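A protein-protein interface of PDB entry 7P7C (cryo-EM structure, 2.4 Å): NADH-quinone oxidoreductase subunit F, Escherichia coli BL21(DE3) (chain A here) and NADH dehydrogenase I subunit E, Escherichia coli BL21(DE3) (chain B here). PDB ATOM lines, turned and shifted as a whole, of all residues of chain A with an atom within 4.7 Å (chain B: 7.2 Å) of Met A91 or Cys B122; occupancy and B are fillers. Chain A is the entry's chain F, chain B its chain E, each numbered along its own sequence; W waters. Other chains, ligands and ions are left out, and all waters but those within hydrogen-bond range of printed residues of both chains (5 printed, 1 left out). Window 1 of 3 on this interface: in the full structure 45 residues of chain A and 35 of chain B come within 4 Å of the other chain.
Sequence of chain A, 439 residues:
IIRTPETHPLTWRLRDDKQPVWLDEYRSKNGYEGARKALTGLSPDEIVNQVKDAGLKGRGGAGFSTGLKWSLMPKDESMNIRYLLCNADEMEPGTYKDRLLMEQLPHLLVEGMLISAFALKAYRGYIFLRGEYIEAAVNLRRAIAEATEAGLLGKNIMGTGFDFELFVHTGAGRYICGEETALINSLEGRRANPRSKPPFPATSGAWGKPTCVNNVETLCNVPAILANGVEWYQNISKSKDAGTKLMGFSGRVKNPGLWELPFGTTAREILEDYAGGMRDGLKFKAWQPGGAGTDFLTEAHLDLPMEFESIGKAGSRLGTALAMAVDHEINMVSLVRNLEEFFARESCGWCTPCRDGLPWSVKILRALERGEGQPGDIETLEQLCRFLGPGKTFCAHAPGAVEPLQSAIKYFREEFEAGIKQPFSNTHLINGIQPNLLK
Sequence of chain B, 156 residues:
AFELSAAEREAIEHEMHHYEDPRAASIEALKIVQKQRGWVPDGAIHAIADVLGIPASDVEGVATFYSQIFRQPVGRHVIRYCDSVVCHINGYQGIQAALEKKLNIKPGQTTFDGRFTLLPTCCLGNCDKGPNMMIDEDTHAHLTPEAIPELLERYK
The side-chain sulfur (SD) of Met A91 is in hydrogen-bond range of the side-chain sulfur (SG) of Cys B122 (3.6 Å). NH2 of Arg A130 sits at hydrogen-bond distance from O of Cys B123 (2.8 Å). The backbone carbonyl oxygen (O) of Gly A173 lies close to the side-chain hydroxyl (OG) of Ser B67 (2.3 Å). The guanidinium group (NH1) of Arg A345 is in salt-bridge range of the side-chain carboxylate (OD2) of Asp B83 (2.6 Å). The backbone NH (N) of Cys B122 sits close to the guanidinium group (NH2) of Arg A345, 3.4 Å away. OE2 of Glu A132 is in salt-bridge range of NH1 of Arg B80.
Water W3 lies within hydrogen-bond range of SG of Cys B122, OG1 of Thr B121 and NH2 of Arg A130. Water W4 lies within hydrogen-bond range of the backbone carbonyl oxygen of Met A91, the backbone carbonyl oxygen of Cys B123 and the side-chain sulfur of Cys B122. Water W2 lies within hydrogen-bond range of the side-chain hydroxyl of Ser B67 (2.9 Å), the backbone carbonyl oxygen of Gly A173 (3.0 Å) and the side-chain sulfur of Cys B122 (3.7 Å). Water W5 lies within hydrogen-bond range of the side-chain sulfur (SG) of Cys B122, the backbone carbonyl oxygen (O) of Gly A173 and the side-chain hydroxyl (OG) of Ser B67. Water W1 lies within hydrogen-bond range of the side-chain carboxylate of Asp B83 (3.0 Å), the guanidinium group of Arg A345 (3.0 Å) and the side-chain hydroxyl of Ser B84 (3.1 Å).
The side-chain sulfur (SD) of Met A91 sits at hydrogen-bond distance from the guanidinium group (NH2) of Arg A130, at 3.7 Å. SG of Cys B123 lies close to N of Gly B125, 3.3 Å away. N of Asp B83 is in hydrogen-bond range of O of Thr B121, 3.2 Å away. The backbone carbonyl oxygen of Tyr B81 sits at hydrogen-bond distance from the backbone NH of Thr B121 (2.9 Å). The guanidinium group (NH1) of Arg A130 sits at hydrogen-bond distance from the backbone carbonyl oxygen (O) of Glu A90. The side-chain amide nitrogen (NE2) of Gln B68 is in hydrogen-bond range of the side-chain hydroxyl (OG) of Ser B67, at 3.4 Å.
Printed residues of chain A that touch a printed residue of chain B: Met A91, Pro A93, Arg A130, Glu A132, Gly A173, Arg A174, Phe A342 and Arg A345. Hydrophobic or aromatic side chains of chain A that line the printed part of chain B: Met A91, Pro A93 and Phe A342. Of the 13 printed residues of chain B, 9 touch a printed residue of chain A. Hydrophobic or aromatic side chains of chain B that line the printed part of chain A: Leu B124. Among the printed residues, 15 pairs touch across the chains. Among the printed residues, Asp or Glu carboxylates within 4 Å of a Lys or Arg side-chain nitrogen of the other chain: Glu A132 with Arg B80 (3.3 Å) and Arg A345 with Asp B83 (2.6 Å).
Of the printed residues of chain B, Met A91 touches Cys B122. Cys B122 touches just these residues of chain A: Met A91 (3.6 Å), Phe A342 (3.7 Å) and Arg A345 (3.4 Å). Of the printed residues of chain B, Arg A345 touches Asp B83 (2.6 Å), Thr B121 (3.4 Å) and Cys B122 (3.4 Å). Of the printed residues of chain A, Cys B123 touches Pro A93 and Arg A130. Printed residues of chain B within 4 Å of Phe A342: Cys B122 (3.7 Å). Ser B84 touches none of the printed residues of chain A. Pro B120 touches none of the printed residues of chain A. The nearest printed residue of chain A that does not touch Cys B122 is Arg A130 (4.7 Å). The nearest printed residue of chain B that does not touch Arg A345 is Pro B120 (4.5 Å).
Among the printed residues, pairs that only touch across the chains: Pro A93 with Cys B123 (3.6 Å), Arg A130 with Leu B124 (3.5 Å), Arg A130 with Gly B125 (3.6 Å), Glu A132 with Gln B68 (3.6 Å), Glu A132 with Leu B124 (3.9 Å), Gly A173 with Gln B68 (3.8 Å), Arg A174 with Ser B67 (3.8 Å), Phe A342 with Cys B122 (3.7 Å) and Arg A345 with Thr B121 (3.4 Å).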
ATOM      1  N   ASP A  89      29.469  -7.178   5.588  1.00  0.00           N
ATOM      2  CA  ASP A  89      28.795  -6.654   4.407  1.00  0.00           C
ATOM      3  C   ASP A  89      27.357  -6.272   4.729  1.00  0.00           C
ATOM      4  O   ASP A  89      26.972  -5.108   4.589  1.00  0.00           O
ATOM      5  CB  ASP A  89      28.851  -7.673   3.269  1.00  0.00           C
ATOM      6  CG  ASP A  89      28.991  -7.016   1.910  1.00  0.00           C
ATOM      7  OD1 ASP A  89      29.486  -5.872   1.849  1.00  0.00           O
ATOM      8  OD2 ASP A  89      28.600  -7.636   0.901  1.00  0.00           O
ATOM      9  N   GLU A  90      26.559  -7.241   5.183  1.00  0.00           N
ATOM     10  CA  GLU A  90      25.184  -7.046   5.658  1.00  0.00           C
ATOM     11  C   GLU A  90      24.319  -6.319   4.628  1.00  0.00           C
ATOM     12  O   GLU A  90      23.747  -5.261   4.887  1.00  0.00           O
ATOM     13  CB  GLU A  90      25.159  -6.312   7.000  1.00  0.00           C
ATOM     14  CG  GLU A  90      23.967  -6.702   7.857  1.00  0.00           C
ATOM     15  CD  GLU A  90      23.661  -5.700   8.946  1.00  0.00           C
ATOM     16  OE1 GLU A  90      23.906  -4.495   8.744  1.00  0.00           O
ATOM     17  OE2 GLU A  90      23.172  -6.124  10.010  1.00  0.00           O
ATOM     18  N   MET A  91      24.247  -6.901   3.440  1.00  0.00           N
ATOM     19  CA  MET A  91      23.495  -6.310   2.348  1.00  0.00           C
ATOM     20  C   MET A  91      22.147  -6.977   2.131  1.00  0.00           C
ATOM     21  O   MET A  91      21.424  -6.592   1.208  1.00  0.00           O
ATOM     22  CB  MET A  91      24.317  -6.361   1.061  1.00  0.00           C
ATOM     23  CG  MET A  91      25.325  -5.249   0.947  1.00  0.00           C
ATOM     24  SD  MET A  91      24.748  -3.914  -0.098  1.00  0.00           S
ATOM     25  CE  MET A  91      26.243  -2.950  -0.215  1.00  0.00           C
ATOM     26  N   GLU A  92      21.801  -7.963   2.944  1.00  0.00           N
ATOM     27  CA  GLU A  92      20.488  -8.584   2.849  1.00  0.00           C
ATOM     28  C   GLU A  92      19.424  -7.596   3.310  1.00  0.00           C
ATOM     29  O   GLU A  92      19.557  -7.018   4.395  1.00  0.00           O
ATOM     30  CB  GLU A  92      20.438  -9.855   3.690  1.00  0.00           C
ATOM     31  CG  GLU A  92      19.070 -10.507   3.762  1.00  0.00           C
ATOM     32  CD  GLU A  92      18.883 -11.596   2.727  1.00  0.00           C
ATOM     33  OE1 GLU A  92      18.988 -11.297   1.521  1.00  0.00           O
ATOM     34  OE2 GLU A  92      18.629 -12.755   3.122  1.00  0.00           O
ATOM     35  N   PRO A  93      18.393  -7.341   2.506  1.00  0.00           N
ATOM     36  CA  PRO A  93      17.334  -6.416   2.925  1.00  0.00           C
ATOM     37  C   PRO A  93      16.583  -6.923   4.144  1.00  0.00           C
ATOM     38  O   PRO A  93      16.245  -8.103   4.246  1.00  0.00           O
ATOM     39  CB  PRO A  93      16.427  -6.338   1.693  1.00  0.00           C
ATOM     40  CG  PRO A  93      17.312  -6.692   0.557  1.00  0.00           C
ATOM     41  CD  PRO A  93      18.268  -7.716   1.091  1.00  0.00           C
ATOM     42  N   ARG A 130      30.707  -2.992   4.435  1.00  0.00           N
ATOM     43  CA  ARG A 130      30.061  -2.288   3.336  1.00  0.00           C
ATOM     44  C   ARG A 130      30.386  -0.797   3.388  1.00  0.00           C
ATOM     45  O   ARG A 130      30.652  -0.231   4.451  1.00  0.00           O
ATOM     46  CB  ARG A 130      28.548  -2.510   3.360  1.00  0.00           C
ATOM     47  CG  ARG A 130      27.790  -1.711   4.403  1.00  0.00           C
ATOM     48  CD  ARG A 130      26.300  -2.007   4.352  1.00  0.00           C
ATOM     49  NE  ARG A 130      25.640  -1.413   3.198  1.00  0.00           N
ATOM     50  CZ  ARG A 130      24.350  -1.551   2.927  1.00  0.00           C
ATOM     51  NH1 ARG A 130      23.555  -2.271   3.699  1.00  0.00           N
ATOM     52  NH2 ARG A 130      23.847  -0.954   1.851  1.00  0.00           N
ATOM     53  N   GLU A 132      28.549   1.815   2.808  1.00  0.00           N
ATOM     54  CA  GLU A 132      27.526   2.713   3.325  1.00  0.00           C
ATOM     55  C   GLU A 132      27.614   2.893   4.834  1.00  0.00           C
ATOM     56  O   GLU A 132      27.022   3.837   5.367  1.00  0.00           O
ATOM     57  CB  GLU A 132      26.134   2.203   2.947  1.00  0.00           C
ATOM     58  CG  GLU A 132      25.794   2.333   1.469  1.00  0.00           C
ATOM     59  CD  GLU A 132      26.415   1.238   0.623  1.00  0.00           C
ATOM     60  OE1 GLU A 132      26.417   0.074   1.069  1.00  0.00           O
ATOM     61  OE2 GLU A 132      26.911   1.542  -0.481  1.00  0.00           O
ATOM     62  N   GLY A 173      29.588  -1.723  -2.826  1.00  0.00           N
ATOM     63  CA  GLY A 173      28.165  -1.779  -3.094  1.00  0.00           C
ATOM     64  C   GLY A 173      27.648  -2.872  -4.007  1.00  0.00           C
ATOM     65  O   GLY A 173      27.076  -2.577  -5.060  1.00  0.00           O
ATOM     66  N   ARG A 174      27.833  -4.131  -3.624  1.00  0.00           N
ATOM     67  CA  ARG A 174      27.160  -5.243  -4.277  1.00  0.00           C
ATOM     68  C   ARG A 174      26.713  -6.235  -3.215  1.00  0.00           C
ATOM     69  O   ARG A 174      27.440  -6.492  -2.252  1.00  0.00           O
ATOM     70  CB  ARG A 174      28.060  -5.941  -5.304  1.00  0.00           C
ATOM     71  CG  ARG A 174      28.102  -5.275  -6.665  1.00  0.00           C
ATOM     72  CD  ARG A 174      26.740  -5.254  -7.326  1.00  0.00           C
ATOM     73  NE  ARG A 174      26.802  -4.635  -8.645  1.00  0.00           N
ATOM     74  CZ  ARG A 174      25.753  -4.185  -9.317  1.00  0.00           C
ATOM     75  NH1 ARG A 174      24.529  -4.272  -8.828  1.00  0.00           N
ATOM     76  NH2 ARG A 174      25.939  -3.631 -10.511  1.00  0.00           N
ATOM     77  N   TYR A 175      25.513  -6.786  -3.396  1.00  0.00           N
ATOM     78  CA  TYR A 175      24.962  -7.714  -2.413  1.00  0.00           C
ATOM     79  C   TYR A 175      25.672  -9.060  -2.437  1.00  0.00           C
ATOM     80  O   TYR A 175      25.784  -9.716  -1.395  1.00  0.00           O
ATOM     81  CB  TYR A 175      23.464  -7.888  -2.659  1.00  0.00           C
ATOM     82  CG  TYR A 175      22.831  -9.059  -1.948  1.00  0.00           C
ATOM     83  CD1 TYR A 175      22.765  -9.104  -0.565  1.00  0.00           C
ATOM     84  CD2 TYR A 175      22.289 -10.114  -2.662  1.00  0.00           C
ATOM     85  CE1 TYR A 175      22.190 -10.166   0.086  1.00  0.00           C
ATOM     86  CE2 TYR A 175      21.705 -11.181  -2.017  1.00  0.00           C
ATOM     87  CZ  TYR A 175      21.659 -11.202  -0.644  1.00  0.00           C
ATOM     88  OH  TYR A 175      21.080 -12.264   0.005  1.00  0.00           O
ATOM     89  N   PHE A 342      15.159  -6.650  -6.828  1.00  0.00           N
ATOM     90  CA  PHE A 342      16.403  -6.624  -6.062  1.00  0.00           C
ATOM     91  C   PHE A 342      17.274  -7.831  -6.385  1.00  0.00           C
ATOM     92  O   PHE A 342      18.469  -7.690  -6.663  1.00  0.00           O
ATOM     93  CB  PHE A 342      16.117  -6.580  -4.559  1.00  0.00           C
ATOM     94  CG  PHE A 342      17.316  -6.917  -3.713  1.00  0.00           C
ATOM     95  CD1 PHE A 342      18.305  -5.975  -3.497  1.00  0.00           C
ATOM     96  CD2 PHE A 342      17.465  -8.177  -3.145  1.00  0.00           C
ATOM     97  CE1 PHE A 342      19.412  -6.274  -2.731  1.00  0.00           C
ATOM     98  CE2 PHE A 342      18.576  -8.483  -2.390  1.00  0.00           C
ATOM     99  CZ  PHE A 342      19.550  -7.527  -2.184  1.00  0.00           C
ATOM    100  N   ARG A 345      18.682  -7.850 -10.038  1.00  0.00           N
ATOM    101  CA  ARG A 345      19.742  -6.885 -10.283  1.00  0.00           C
ATOM    102  C   ARG A 345      20.969  -7.100  -9.401  1.00  0.00           C
ATOM    103  O   ARG A 345      21.999  -6.467  -9.642  1.00  0.00           O
ATOM    104  CB  ARG A 345      19.212  -5.462 -10.115  1.00  0.00           C
ATOM    105  CG  ARG A 345      19.280  -4.910  -8.716  1.00  0.00           C
ATOM    106  CD  ARG A 345      18.513  -3.613  -8.643  1.00  0.00           C
ATOM    107  NE  ARG A 345      18.748  -2.903  -7.395  1.00  0.00           N
ATOM    108  CZ  ARG A 345      17.920  -2.001  -6.890  1.00  0.00           C
ATOM    109  NH1 ARG A 345      16.789  -1.687  -7.498  1.00  0.00           N
ATOM    110  NH2 ARG A 345      18.236  -1.398  -5.748  1.00  0.00           N
ATOM    111  N   SER B  67      28.479  -1.302  -8.113  1.00  0.00           N
ATOM    112  CA  SER B  67      27.534  -0.242  -8.443  1.00  0.00           C
ATOM    113  C   SER B  67      27.959   1.106  -7.879  1.00  0.00           C
ATOM    114  O   SER B  67      27.604   2.147  -8.443  1.00  0.00           O
ATOM    115  CB  SER B  67      26.141  -0.613  -7.940  1.00  0.00           C
ATOM    116  OG  SER B  67      26.187  -1.053  -6.596  1.00  0.00           O
ATOM    117  N   GLN B  68      28.711   1.121  -6.781  1.00  0.00           N
ATOM    118  CA  GLN B  68      29.105   2.382  -6.169  1.00  0.00           C
ATOM    119  C   GLN B  68      30.353   2.987  -6.792  1.00  0.00           C
ATOM    120  O   GLN B  68      30.750   4.086  -6.397  1.00  0.00           O
ATOM    121  CB  GLN B  68      29.312   2.202  -4.665  1.00  0.00           C
ATOM    122  CG  GLN B  68      28.029   1.958  -3.892  1.00  0.00           C
ATOM    123  CD  GLN B  68      26.842   2.697  -4.479  1.00  0.00           C
ATOM    124  OE1 GLN B  68      26.791   3.927  -4.461  1.00  0.00           O
ATOM    125  NE2 GLN B  68      25.878   1.949  -4.997  1.00  0.00           N
ATOM    126  N   ARG B  80      20.843   8.745  -3.007  1.00  0.00           N
ATOM    127  CA  ARG B  80      20.651   7.309  -3.177  1.00  0.00           C
ATOM    128  C   ARG B  80      19.499   6.893  -2.274  1.00  0.00           C
ATOM    129  O   ARG B  80      19.674   6.750  -1.061  1.00  0.00           O
ATOM    130  CB  ARG B  80      21.927   6.541  -2.855  1.00  0.00           C
ATOM    131  CG  ARG B  80      22.986   6.656  -3.929  1.00  0.00           C
ATOM    132  CD  ARG B  80      24.023   5.567  -3.793  1.00  0.00           C
ATOM    133  NE  ARG B  80      24.880   5.773  -2.633  1.00  0.00           N
ATOM    134  CZ  ARG B  80      25.201   4.825  -1.764  1.00  0.00           C
ATOM    135  NH1 ARG B  80      24.752   3.588  -1.893  1.00  0.00           N
ATOM    136  NH2 ARG B  80      25.995   5.127  -0.741  1.00  0.00           N
ATOM    137  N   TYR B  81      18.328   6.694  -2.864  1.00  0.00           N
ATOM    138  CA  TYR B  81      17.157   6.306  -2.092  1.00  0.00           C
ATOM    139  C   TYR B  81      17.009   4.792  -2.101  1.00  0.00           C
ATOM    140  O   TYR B  81      17.223   4.140  -3.125  1.00  0.00           O
ATOM    141  CB  TYR B  81      15.887   6.977  -2.628  1.00  0.00           C
ATOM    142  CG  TYR B  81      15.467   6.553  -4.018  1.00  0.00           C
ATOM    143  CD1 TYR B  81      16.003   7.165  -5.141  1.00  0.00           C
ATOM    144  CD2 TYR B  81      14.521   5.553  -4.203  1.00  0.00           C
ATOM    145  CE1 TYR B  81      15.622   6.782  -6.409  1.00  0.00           C
ATOM    146  CE2 TYR B  81      14.137   5.164  -5.466  1.00  0.00           C
ATOM    147  CZ  TYR B  81      14.688   5.782  -6.564  1.00  0.00           C
ATOM    148  OH  TYR B  81      14.303   5.396  -7.824  1.00  0.00           O
ATOM    149  N   CYS B  82      16.662   4.235  -0.948  1.00  0.00           N
ATOM    150  CA  CYS B  82      16.488   2.798  -0.826  1.00  0.00           C
ATOM    151  C   CYS B  82      15.174   2.375  -1.467  1.00  0.00           C
ATOM    152  O   CYS B  82      14.112   2.904  -1.129  1.00  0.00           O
ATOM    153  CB  CYS B  82      16.520   2.383   0.642  1.00  0.00           C
ATOM    154  SG  CYS B  82      16.242   0.633   0.909  1.00  0.00           S
ATOM    155  N   ASP B  83      15.243   1.417  -2.393  1.00  0.00           N
ATOM    156  CA  ASP B  83      14.049   0.886  -3.037  1.00  0.00           C
ATOM    157  C   ASP B  83      13.800  -0.571  -2.664  1.00  0.00           C
ATOM    158  O   ASP B  83      13.114  -1.286  -3.398  1.00  0.00           O
ATOM    159  CB  ASP B  83      14.131   1.047  -4.560  1.00  0.00           C
ATOM    160  CG  ASP B  83      15.188   0.173  -5.200  1.00  0.00           C
ATOM    161  OD1 ASP B  83      16.261  -0.016  -4.610  1.00  0.00           O
ATOM    162  OD2 ASP B  83      14.940  -0.319  -6.318  1.00  0.00           O
ATOM    163  N   SER B  84      14.333  -1.018  -1.531  1.00  0.00           N
ATOM    164  CA  SER B  84      14.216  -2.411  -1.125  1.00  0.00           C
ATOM    165  C   SER B  84      12.884  -2.639  -0.414  1.00  0.00           C
ATOM    166  O   SER B  84      12.028  -1.754  -0.343  1.00  0.00           O
ATOM    167  CB  SER B  84      15.410  -2.812  -0.267  1.00  0.00           C
ATOM    168  OG  SER B  84      16.537  -3.093  -1.076  1.00  0.00           O
ATOM    169  N   PRO B 120      18.416   4.911  -7.346  1.00  0.00           N
ATOM    170  CA  PRO B 120      17.945   3.878  -6.426  1.00  0.00           C
ATOM    171  C   PRO B 120      19.114   3.029  -5.960  1.00  0.00           C
ATOM    172  O   PRO B 120      20.084   2.809  -6.687  1.00  0.00           O
ATOM    173  CB  PRO B 120      16.963   3.066  -7.274  1.00  0.00           C
ATOM    174  CG  PRO B 120      17.464   3.230  -8.661  1.00  0.00           C
ATOM    175  CD  PRO B 120      18.069   4.608  -8.744  1.00  0.00           C
ATOM    176  N   THR B 121      19.020   2.560  -4.723  1.00  0.00           N
ATOM    177  CA  THR B 121      20.067   1.736  -4.147  1.00  0.00           C
ATOM    178  C   THR B 121      19.424   0.627  -3.334  1.00  0.00           C
ATOM    179  O   THR B 121      18.286   0.742  -2.879  1.00  0.00           O
ATOM    180  CB  THR B 121      21.029   2.559  -3.274  1.00  0.00           C
ATOM    181  OG1 THR B 121      22.114   1.730  -2.846  1.00  0.00           O
ATOM    182  CG2 THR B 121      20.318   3.123  -2.054  1.00  0.00           C
ATOM    183  N   CYS B 122      20.182  -0.448  -3.134  1.00  0.00           N
ATOM    184  CA  CYS B 122      19.708  -1.558  -2.324  1.00  0.00           C
ATOM    185  C   CYS B 122      19.634  -1.141  -0.855  1.00  0.00           C
ATOM    186  O   CYS B 122      19.934  -0.001  -0.485  1.00  0.00           O
ATOM    187  CB  CYS B 122      20.609  -2.775  -2.517  1.00  0.00           C
ATOM    188  SG  CYS B 122      22.371  -2.438  -2.341  1.00  0.00           S
ATOM    189  N   CYS B 123      19.227  -2.089  -0.013  1.00  0.00           N
ATOM    190  CA  CYS B 123      18.907  -1.799   1.381  1.00  0.00           C
ATOM    191  C   CYS B 123      20.115  -1.254   2.132  1.00  0.00           C
ATOM    192  O   CYS B 123      21.216  -1.803   2.054  1.00  0.00           O
ATOM    193  CB  CYS B 123      18.388  -3.060   2.062  1.00  0.00           C
ATOM    194  SG  CYS B 123      18.558  -3.068   3.851  1.00  0.00           S
ATOM    195  N   LEU B 124      19.896  -0.159   2.852  1.00  0.00           N
ATOM    196  CA  LEU B 124      20.956   0.585   3.514  1.00  0.00           C
ATOM    197  C   LEU B 124      21.232   0.093   4.926  1.00  0.00           C
ATOM    198  O   LEU B 124      22.021   0.718   5.639  1.00  0.00           O
ATOM    199  CB  LEU B 124      20.606   2.074   3.544  1.00  0.00           C
ATOM    200  CG  LEU B 124      20.516   2.764   2.184  1.00  0.00           C
ATOM    201  CD1 LEU B 124      19.924   4.151   2.327  1.00  0.00           C
ATOM    202  CD2 LEU B 124      21.882   2.827   1.532  1.00  0.00           C
ATOM    203  N   GLY B 125      20.609  -1.004   5.341  1.00  0.00           N
ATOM    204  CA  GLY B 125      20.775  -1.502   6.693  1.00  0.00           C
ATOM    205  C   GLY B 125      20.201  -0.584   7.748  1.00  0.00           C
ATOM    206  O   GLY B 125      20.771  -0.465   8.839  1.00  0.00           O
HETATM  207  O   HOH W   1      16.220  -3.011  -4.132  1.00  0.00           O
HETATM  208  O   HOH W   2      24.171  -2.856  -5.527  1.00  0.00           O
HETATM  209  O   HOH W   3      23.257  -0.216  -1.106  1.00  0.00           O
HETATM  210  O   HOH W   4      21.958  -4.125   0.199  1.00  0.00           O
HETATM  211  O   HOH W   5      24.906  -1.234  -3.353  1.00  0.00           O
